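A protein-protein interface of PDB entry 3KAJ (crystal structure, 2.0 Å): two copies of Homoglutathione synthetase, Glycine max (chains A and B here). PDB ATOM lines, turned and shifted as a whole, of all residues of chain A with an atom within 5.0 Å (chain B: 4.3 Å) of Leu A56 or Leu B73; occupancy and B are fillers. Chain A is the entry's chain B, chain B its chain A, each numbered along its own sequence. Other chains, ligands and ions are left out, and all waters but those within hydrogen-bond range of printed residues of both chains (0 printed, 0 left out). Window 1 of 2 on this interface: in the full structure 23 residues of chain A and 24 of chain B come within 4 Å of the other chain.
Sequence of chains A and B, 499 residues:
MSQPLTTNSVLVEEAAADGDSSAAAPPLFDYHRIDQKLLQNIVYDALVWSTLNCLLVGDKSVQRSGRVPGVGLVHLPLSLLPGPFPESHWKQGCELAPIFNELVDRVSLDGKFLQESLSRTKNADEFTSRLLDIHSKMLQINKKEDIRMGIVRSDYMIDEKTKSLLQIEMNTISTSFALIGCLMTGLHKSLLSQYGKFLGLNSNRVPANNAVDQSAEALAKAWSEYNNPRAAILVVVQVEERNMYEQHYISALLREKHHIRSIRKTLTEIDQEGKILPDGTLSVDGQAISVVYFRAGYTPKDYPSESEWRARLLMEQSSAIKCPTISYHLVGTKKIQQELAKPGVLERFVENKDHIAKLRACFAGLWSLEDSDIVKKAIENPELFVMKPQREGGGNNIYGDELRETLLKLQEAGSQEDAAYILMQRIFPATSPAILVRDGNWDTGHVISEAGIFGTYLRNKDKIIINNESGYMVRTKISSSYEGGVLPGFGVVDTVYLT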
ATOM      1  N   SER A  50     -18.663  29.869  -7.426  1.00  0.00           N
ATOM      2  CA  SER A  50     -18.919  29.078  -6.208  1.00  0.00           C
ATOM      3  C   SER A  50     -18.068  27.848  -6.197  1.00  0.00           C
ATOM      4  O   SER A  50     -17.484  27.486  -5.158  1.00  0.00           O
ATOM      5  CB  SER A  50     -20.395  28.604  -6.192  1.00  0.00           C
ATOM      6  OG  SER A  50     -21.276  29.701  -5.942  1.00  0.00           O
ATOM      7  N   THR A  51     -18.041  27.156  -7.340  1.00  0.00           N
ATOM      8  CA  THR A  51     -17.198  25.941  -7.425  1.00  0.00           C
ATOM      9  C   THR A  51     -15.708  26.270  -7.260  1.00  0.00           C
ATOM     10  O   THR A  51     -15.054  25.682  -6.388  1.00  0.00           O
ATOM     11  CB  THR A  51     -17.466  25.111  -8.660  1.00  0.00           C
ATOM     12  OG1 THR A  51     -18.898  24.952  -8.839  1.00  0.00           O
ATOM     13  CG2 THR A  51     -16.715  23.721  -8.565  1.00  0.00           C
ATOM     14  N   CYS A  54     -14.868  27.372  -3.391  1.00  0.00           N
ATOM     15  CA  CYS A  54     -15.352  26.556  -2.275  1.00  0.00           C
ATOM     16  C   CYS A  54     -16.528  27.125  -1.495  1.00  0.00           C
ATOM     17  O   CYS A  54     -16.581  27.005  -0.286  1.00  0.00           O
ATOM     18  CB  CYS A  54     -14.242  26.147  -1.284  1.00  0.00           C
ATOM     19  SG  CYS A  54     -14.685  24.508  -0.532  1.00  0.00           S
ATOM     20  N   LEU A  55     -17.502  27.658  -2.225  1.00  0.00           N
ATOM     21  CA  LEU A  55     -18.797  28.022  -1.678  1.00  0.00           C
ATOM     22  C   LEU A  55     -19.611  26.764  -1.935  1.00  0.00           C
ATOM     23  O   LEU A  55     -20.510  26.740  -2.761  1.00  0.00           O
ATOM     24  CB  LEU A  55     -19.350  29.247  -2.431  1.00  0.00           C
ATOM     25  CG  LEU A  55     -20.613  29.958  -1.917  1.00  0.00           C
ATOM     26  CD1 LEU A  55     -20.495  30.327  -0.384  1.00  0.00           C
ATOM     27  CD2 LEU A  55     -20.788  31.178  -2.800  1.00  0.00           C
ATOM     28  N   LEU A  56     -19.257  25.724  -1.193  1.00  0.00           N
ATOM     29  CA  LEU A  56     -19.694  24.340  -1.483  1.00  0.00           C
ATOM     30  C   LEU A  56     -20.043  23.679  -0.190  1.00  0.00           C
ATOM     31  O   LEU A  56     -19.429  23.953   0.845  1.00  0.00           O
ATOM     32  CB  LEU A  56     -18.531  23.565  -2.145  1.00  0.00           C
ATOM     33  CG  LEU A  56     -18.093  23.954  -3.533  1.00  0.00           C
ATOM     34  CD1 LEU A  56     -16.803  23.163  -3.971  1.00  0.00           C
ATOM     35  CD2 LEU A  56     -19.317  23.643  -4.493  1.00  0.00           C
ATOM     36  N   VAL A  57     -21.047  22.810  -0.230  1.00  0.00           N
ATOM     37  CA  VAL A  57     -21.391  21.961   0.905  1.00  0.00           C
ATOM     38  C   VAL A  57     -21.651  20.537   0.435  1.00  0.00           C
ATOM     39  O   VAL A  57     -21.879  20.287  -0.751  1.00  0.00           O
ATOM     40  CB  VAL A  57     -22.671  22.406   1.670  1.00  0.00           C
ATOM     41  CG1 VAL A  57     -22.344  23.526   2.644  1.00  0.00           C
ATOM     42  CG2 VAL A  57     -23.779  22.720   0.711  1.00  0.00           C
ATOM     43  N   GLY A  58     -21.603  19.614   1.379  1.00  0.00           N
ATOM     44  CA  GLY A  58     -22.080  18.254   1.174  1.00  0.00           C
ATOM     45  C   GLY A  58     -23.547  18.371   0.807  1.00  0.00           C
ATOM     46  O   GLY A  58     -24.307  19.131   1.422  1.00  0.00           O
ATOM     47  N   GLY A  70     -14.832  15.671  -0.082  1.00  0.00           N
ATOM     48  CA  GLY A  70     -14.427  15.493  -1.465  1.00  0.00           C
ATOM     49  C   GLY A  70     -15.493  14.817  -2.283  1.00  0.00           C
ATOM     50  O   GLY A  70     -15.295  14.647  -3.475  1.00  0.00           O
ATOM     51  N   VAL A  71     -16.587  14.370  -1.653  1.00  0.00           N
ATOM     52  CA  VAL A  71     -17.652  13.646  -2.332  1.00  0.00           C
ATOM     53  C   VAL A  71     -19.031  14.295  -2.154  1.00  0.00           C
ATOM     54  O   VAL A  71     -19.290  15.005  -1.160  1.00  0.00           O
ATOM     55  CB  VAL A  71     -17.702  12.128  -1.942  1.00  0.00           C
ATOM     56  CG1 VAL A  71     -16.313  11.493  -2.032  1.00  0.00           C
ATOM     57  CG2 VAL A  71     -18.298  11.909  -0.590  1.00  0.00           C
ATOM     58  N   GLY A  72     -19.909  14.093  -3.131  1.00  0.00           N
ATOM     59  CA  GLY A  72     -21.269  14.637  -3.117  1.00  0.00           C
ATOM     60  C   GLY A  72     -21.350  16.118  -2.777  1.00  0.00           C
ATOM     61  O   GLY A  72     -22.099  16.510  -1.911  1.00  0.00           O
ATOM     62  N   LEU A  73     -20.573  16.927  -3.483  1.00  0.00           N
ATOM     63  CA  LEU A  73     -20.485  18.369  -3.271  1.00  0.00           C
ATOM     64  C   LEU A  73     -21.463  19.156  -4.114  1.00  0.00           C
ATOM     65  O   LEU A  73     -21.705  18.789  -5.249  1.00  0.00           O
ATOM     66  CB  LEU A  73     -19.085  18.813  -3.676  1.00  0.00           C
ATOM     67  CG  LEU A  73     -18.017  18.270  -2.741  1.00  0.00           C
ATOM     68  CD1 LEU A  73     -16.643  18.312  -3.416  1.00  0.00           C
ATOM     69  CD2 LEU A  73     -18.100  19.061  -1.430  1.00  0.00           C
ATOM     70  N   VAL A  74     -22.026  20.249  -3.570  1.00  0.00           N
ATOM     71  CA  VAL A  74     -22.953  21.112  -4.318  1.00  0.00           C
ATOM     72  C   VAL A  74     -22.755  22.560  -3.814  1.00  0.00           C
ATOM     73  O   VAL A  74     -22.324  22.768  -2.687  1.00  0.00           O
ATOM     74  CB  VAL A  74     -24.449  20.651  -4.182  1.00  0.00           C
ATOM     75  CG1 VAL A  74     -24.936  20.852  -2.733  1.00  0.00           C
ATOM     76  CG2 VAL A  74     -25.396  21.445  -5.210  1.00  0.00           C
ATOM     77  N   HIS A  75     -22.967  23.561  -4.653  1.00  0.00           N
ATOM     78  CA  HIS A  75     -22.817  24.924  -4.209  1.00  0.00           C
ATOM     79  C   HIS A  75     -23.806  25.199  -3.034  1.00  0.00           C
ATOM     80  O   HIS A  75     -24.835  24.575  -2.971  1.00  0.00           O
ATOM     81  CB  HIS A  75     -23.091  25.894  -5.396  1.00  0.00           C
ATOM     82  CG  HIS A  75     -24.516  25.853  -5.891  1.00  0.00           C
ATOM     83  ND1 HIS A  75     -25.476  26.752  -5.477  1.00  0.00           N
ATOM     84  CD2 HIS A  75     -25.147  24.980  -6.720  1.00  0.00           C
ATOM     85  CE1 HIS A  75     -26.638  26.453  -6.051  1.00  0.00           C
ATOM     86  NE2 HIS A  75     -26.464  25.378  -6.808  1.00  0.00           N
ATOM     87  N   LEU A  76     -23.497  26.143  -2.147  1.00  0.00           N
ATOM     88  CA  LEU A  76     -24.455  26.576  -1.114  1.00  0.00           C
ATOM     89  C   LEU A  76     -25.727  27.140  -1.745  1.00  0.00           C
ATOM     90  O   LEU A  76     -25.640  27.856  -2.703  1.00  0.00           O
ATOM     91  CB  LEU A  76     -23.846  27.704  -0.265  1.00  0.00           C
ATOM     92  CG  LEU A  76     -23.130  27.475   1.063  1.00  0.00           C
ATOM     93  CD1 LEU A  76     -24.080  26.883   2.113  1.00  0.00           C
ATOM     94  CD2 LEU A  76     -21.902  26.612   0.802  1.00  0.00           C
ATOM     95  N   ARG A 242     -22.046  18.532   6.800  1.00  0.00           N
ATOM     96  CA  ARG A 242     -22.081  18.883   5.367  1.00  0.00           C
ATOM     97  C   ARG A 242     -21.527  20.282   5.059  1.00  0.00           C
ATOM     98  O   ARG A 242     -21.214  20.603   3.908  1.00  0.00           O
ATOM     99  CB  ARG A 242     -23.521  18.763   4.869  1.00  0.00           C
ATOM    100  CG  ARG A 242     -24.107  17.362   5.081  1.00  0.00           C
ATOM    101  CD  ARG A 242     -25.314  17.082   4.164  1.00  0.00           C
ATOM    102  NE  ARG A 242     -25.278  15.713   3.656  1.00  0.00           N
ATOM    103  CZ  ARG A 242     -25.343  14.593   4.390  1.00  0.00           C
ATOM    104  NH1 ARG A 242     -25.284  13.426   3.782  1.00  0.00           N
ATOM    105  NH2 ARG A 242     -25.459  14.614   5.717  1.00  0.00           N
ATOM    106  N   TYR A 245     -16.314  22.077   5.322  1.00  0.00           N
ATOM    107  CA  TYR A 245     -15.293  22.877   4.664  1.00  0.00           C
ATOM    108  C   TYR A 245     -15.029  24.245   5.271  1.00  0.00           C
ATOM    109  O   TYR A 245     -13.885  24.652   5.305  1.00  0.00           O
ATOM    110  CB  TYR A 245     -15.532  22.891   3.155  1.00  0.00           C
ATOM    111  CG  TYR A 245     -15.764  21.467   2.699  1.00  0.00           C
ATOM    112  CD1 TYR A 245     -17.053  21.008   2.478  1.00  0.00           C
ATOM    113  CD2 TYR A 245     -14.712  20.593   2.541  1.00  0.00           C
ATOM    114  CE1 TYR A 245     -17.298  19.705   2.137  1.00  0.00           C
ATOM    115  CE2 TYR A 245     -14.944  19.271   2.149  1.00  0.00           C
ATOM    116  CZ  TYR A 245     -16.253  18.859   1.933  1.00  0.00           C
ATOM    117  OH  TYR A 245     -16.556  17.610   1.550  1.00  0.00           O
ATOM    118  N   LEU B  56     -11.508  19.382  -8.315  1.00  0.00           N
ATOM    119  CA  LEU B  56     -12.857  18.846  -8.401  1.00  0.00           C
ATOM    120  C   LEU B  56     -13.218  18.726  -9.848  1.00  0.00           C
ATOM    121  O   LEU B  56     -12.802  19.545 -10.676  1.00  0.00           O
ATOM    122  CB  LEU B  56     -13.861  19.812  -7.757  1.00  0.00           C
ATOM    123  CG  LEU B  56     -13.600  20.248  -6.311  1.00  0.00           C
ATOM    124  CD1 LEU B  56     -14.598  21.289  -5.832  1.00  0.00           C
ATOM    125  CD2 LEU B  56     -13.565  19.038  -5.415  1.00  0.00           C
ATOM    126  N   VAL B  57     -13.986  17.707 -10.175  1.00  0.00           N
ATOM    127  CA  VAL B  57     -14.592  17.678 -11.524  1.00  0.00           C
ATOM    128  C   VAL B  57     -16.062  17.299 -11.361  1.00  0.00           C
ATOM    129  O   VAL B  57     -16.455  16.708 -10.305  1.00  0.00           O
ATOM    130  CB  VAL B  57     -13.902  16.591 -12.397  1.00  0.00           C
ATOM    131  CG1 VAL B  57     -12.634  17.163 -13.023  1.00  0.00           C
ATOM    132  CG2 VAL B  57     -13.564  15.340 -11.539  1.00  0.00           C
ATOM    133  N   GLY B  58     -16.870  17.525 -12.384  1.00  0.00           N
ATOM    134  CA  GLY B  58     -18.269  16.981 -12.359  1.00  0.00           C
ATOM    135  C   GLY B  58     -18.154  15.474 -12.212  1.00  0.00           C
ATOM    136  O   GLY B  58     -17.279  14.841 -12.849  1.00  0.00           O
ATOM    137  N   GLY B  70     -21.247  23.780 -10.486  1.00  0.00           N
ATOM    138  CA  GLY B  70     -21.737  23.870  -9.118  1.00  0.00           C
ATOM    139  C   GLY B  70     -22.518  22.659  -8.663  1.00  0.00           C
ATOM    140  O   GLY B  70     -22.864  22.577  -7.518  1.00  0.00           O
ATOM    141  N   VAL B  71     -22.844  21.735  -9.563  1.00  0.00           N
ATOM    142  CA  VAL B  71     -23.582  20.528  -9.160  1.00  0.00           C
ATOM    143  C   VAL B  71     -22.827  19.235  -9.451  1.00  0.00           C
ATOM    144  O   VAL B  71     -22.153  19.115 -10.456  1.00  0.00           O
ATOM    145  CB  VAL B  71     -25.013  20.457  -9.796  1.00  0.00           C
ATOM    146  CG1 VAL B  71     -25.771  21.747  -9.571  1.00  0.00           C
ATOM    147  CG2 VAL B  71     -24.960  20.149 -11.214  1.00  0.00           C
ATOM    148  N   GLY B  72     -22.966  18.258  -8.562  1.00  0.00           N
ATOM    149  CA  GLY B  72     -22.486  16.908  -8.832  1.00  0.00           C
ATOM    150  C   GLY B  72     -20.968  16.827  -8.847  1.00  0.00           C
ATOM    151  O   GLY B  72     -20.390  16.253  -9.744  1.00  0.00           O
ATOM    152  N   LEU B  73     -20.329  17.367  -7.831  1.00  0.00           N
ATOM    153  CA  LEU B  73     -18.873  17.426  -7.824  1.00  0.00           C
ATOM    154  C   LEU B  73     -18.281  16.334  -6.960  1.00  0.00           C
ATOM    155  O   LEU B  73     -18.862  15.929  -5.937  1.00  0.00           O
ATOM    156  CB  LEU B  73     -18.405  18.800  -7.340  1.00  0.00           C
ATOM    157  CG  LEU B  73     -18.989  19.961  -8.184  1.00  0.00           C
ATOM    158  CD1 LEU B  73     -19.184  21.177  -7.295  1.00  0.00           C
ATOM    159  CD2 LEU B  73     -18.057  20.264  -9.317  1.00  0.00           C
ATOM    160  N   VAL B  74     -17.076  15.925  -7.357  1.00  0.00           N
ATOM    161  CA  VAL B  74     -16.246  14.960  -6.644  1.00  0.00           C
ATOM    162  C   VAL B  74     -14.766  15.352  -6.898  1.00  0.00           C
ATOM    163  O   VAL B  74     -14.423  15.957  -7.903  1.00  0.00           O
ATOM    164  CB  VAL B  74     -16.514  13.552  -7.199  1.00  0.00           C
ATOM    165  CG1 VAL B  74     -15.887  13.390  -8.604  1.00  0.00           C
ATOM    166  CG2 VAL B  74     -16.072  12.436  -6.232  1.00  0.00           C
ATOM    167  N   TYR B 245     -13.892  23.277 -14.784  1.00  0.00           N
ATOM    168  CA  TYR B 245     -13.372  24.252 -13.806  1.00  0.00           C
ATOM    169  C   TYR B 245     -12.004  24.755 -14.179  1.00  0.00           C
ATOM    170  O   TYR B 245     -11.647  25.916 -13.937  1.00  0.00           O
ATOM    171  CB  TYR B 245     -13.446  23.670 -12.366  1.00  0.00           C
ATOM    172  CG  TYR B 245     -14.863  23.367 -12.133  1.00  0.00           C
ATOM    173  CD1 TYR B 245     -15.332  22.063 -12.255  1.00  0.00           C
ATOM    174  CD2 TYR B 245     -15.772  24.387 -12.054  1.00  0.00           C
ATOM    175  CE1 TYR B 245     -16.656  21.772 -12.137  1.00  0.00           C
ATOM    176  CE2 TYR B 245     -17.144  24.104 -11.919  1.00  0.00           C
ATOM    177  CZ  TYR B 245     -17.562  22.786 -11.979  1.00  0.00           C
ATOM    178  OH  TYR B 245     -18.895  22.457 -11.894  1.00  0.00           O
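OG1 of Thr A51 sits close to N of Gly B70, 3.1 Å away.
O of Gly B70 lies within hydrogen-bond range of N of His A75, 3.0 Å away.
O of Leu B73 sits at hydrogen-bond distance from N of Leu A73, 3.2 Å away.
The backbone NH (N) of Val B57 sits at hydrogen-bond distance from the backbone carbonyl oxygen (O) of Val B74, at 2.9 Å.
The side-chain hydroxyl of Tyr B245 sits at hydrogen-bond distance from the backbone NH of Gly B70, 3.0 Å away.
N of Val A57 is in hydrogen-bond range of O of Val A74 (2.8 Å).
The backbone NH of Gly A70 is in hydrogen-bond range of the side-chain hydroxyl of Tyr A245 (3.1 Å).
Leu B73 touches Thr A51 (CD1 to CG2, 3.8 Å).
CG2 of Thr A51 touches CE2 of Tyr B245, at 3.4 Å.
Leu A56 touches Leu B56.
Leu A56 touches Leu B73.
O of Gly A70 touches CA of Val B74 (3.3 Å).
O of Leu B73 touches N of Gly A72, 3.5 Å away.
Leu A73 touches Leu B56 (CD1 to CD2, 3.7 Å).
Leu A73 touches Gly B72 (O to N, 3.6 Å).
O of Gly B70 touches CA of Val A74, at 3.5 Å.
Leu A56 touches two residues of chain B.
Printed residues of chain A within 4 Å of Leu B73: Thr A51, Leu A56, Gly A72 and Leu A73.
Of the printed residues of chain B, Gly A72 touches Leu B73 (3.5 Å).
Printed residues of chain A within 4 Å of Gly B72: Leu A73 (3.6 Å).
Of the printed residues of chain B, Leu A73 touches Leu B56, Gly B72 and Leu B73.
Of the printed residues of chain B, His A75 touches Gly B70.
Of the printed residues of chain A, Gly B70 touches Thr A51, Val A74 and His A75.
The nearest printed residue of chain B that does not touch Leu A56 is Gly B70 (4.8 Å).
The nearest residue of chain A that does not touch Leu B73 is Val A71 (4.1 Å).
The nearest printed residue of chain A that does not touch Gly B70 is Leu A73 (4.6 Å).
Hydrophobic or aromatic side chains of chain A that line the printed part of chain B: Leu A56, Leu A73, Val A74 and His A75.
Along chain A the printed residues that touch a printed residue of chain B span positions 51 to 75.
Of the 9 printed residues of chain B, 6 touch a printed residue of chain A.
Printed residues of chain B that touch a printed residue of chain A: Leu B56, Gly B70, Gly B72, Leu B73, Val B74 and Tyr B245.
Among the printed residues, 12 pairs touch across the chains.
Among the printed residues, no Asp or Glu carboxylate lies within 4 Å of a Lys or Arg side-chain nitrogen of the other chain.
Leu A56 touches its own counterpart, Leu B56.
Leu A56 touches Leu B73, and with the chains exchanged Leu A73 touches Leu B56.
Gly A70 touches Val B74, and with the chains exchanged Val A74 touches Gly B70.
Leu B73 touches its own counterpart, Leu A73.
Of the 12 pairs that touch across the chains among the printed residues, 8 have their exchanged pair printed and touching as well.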
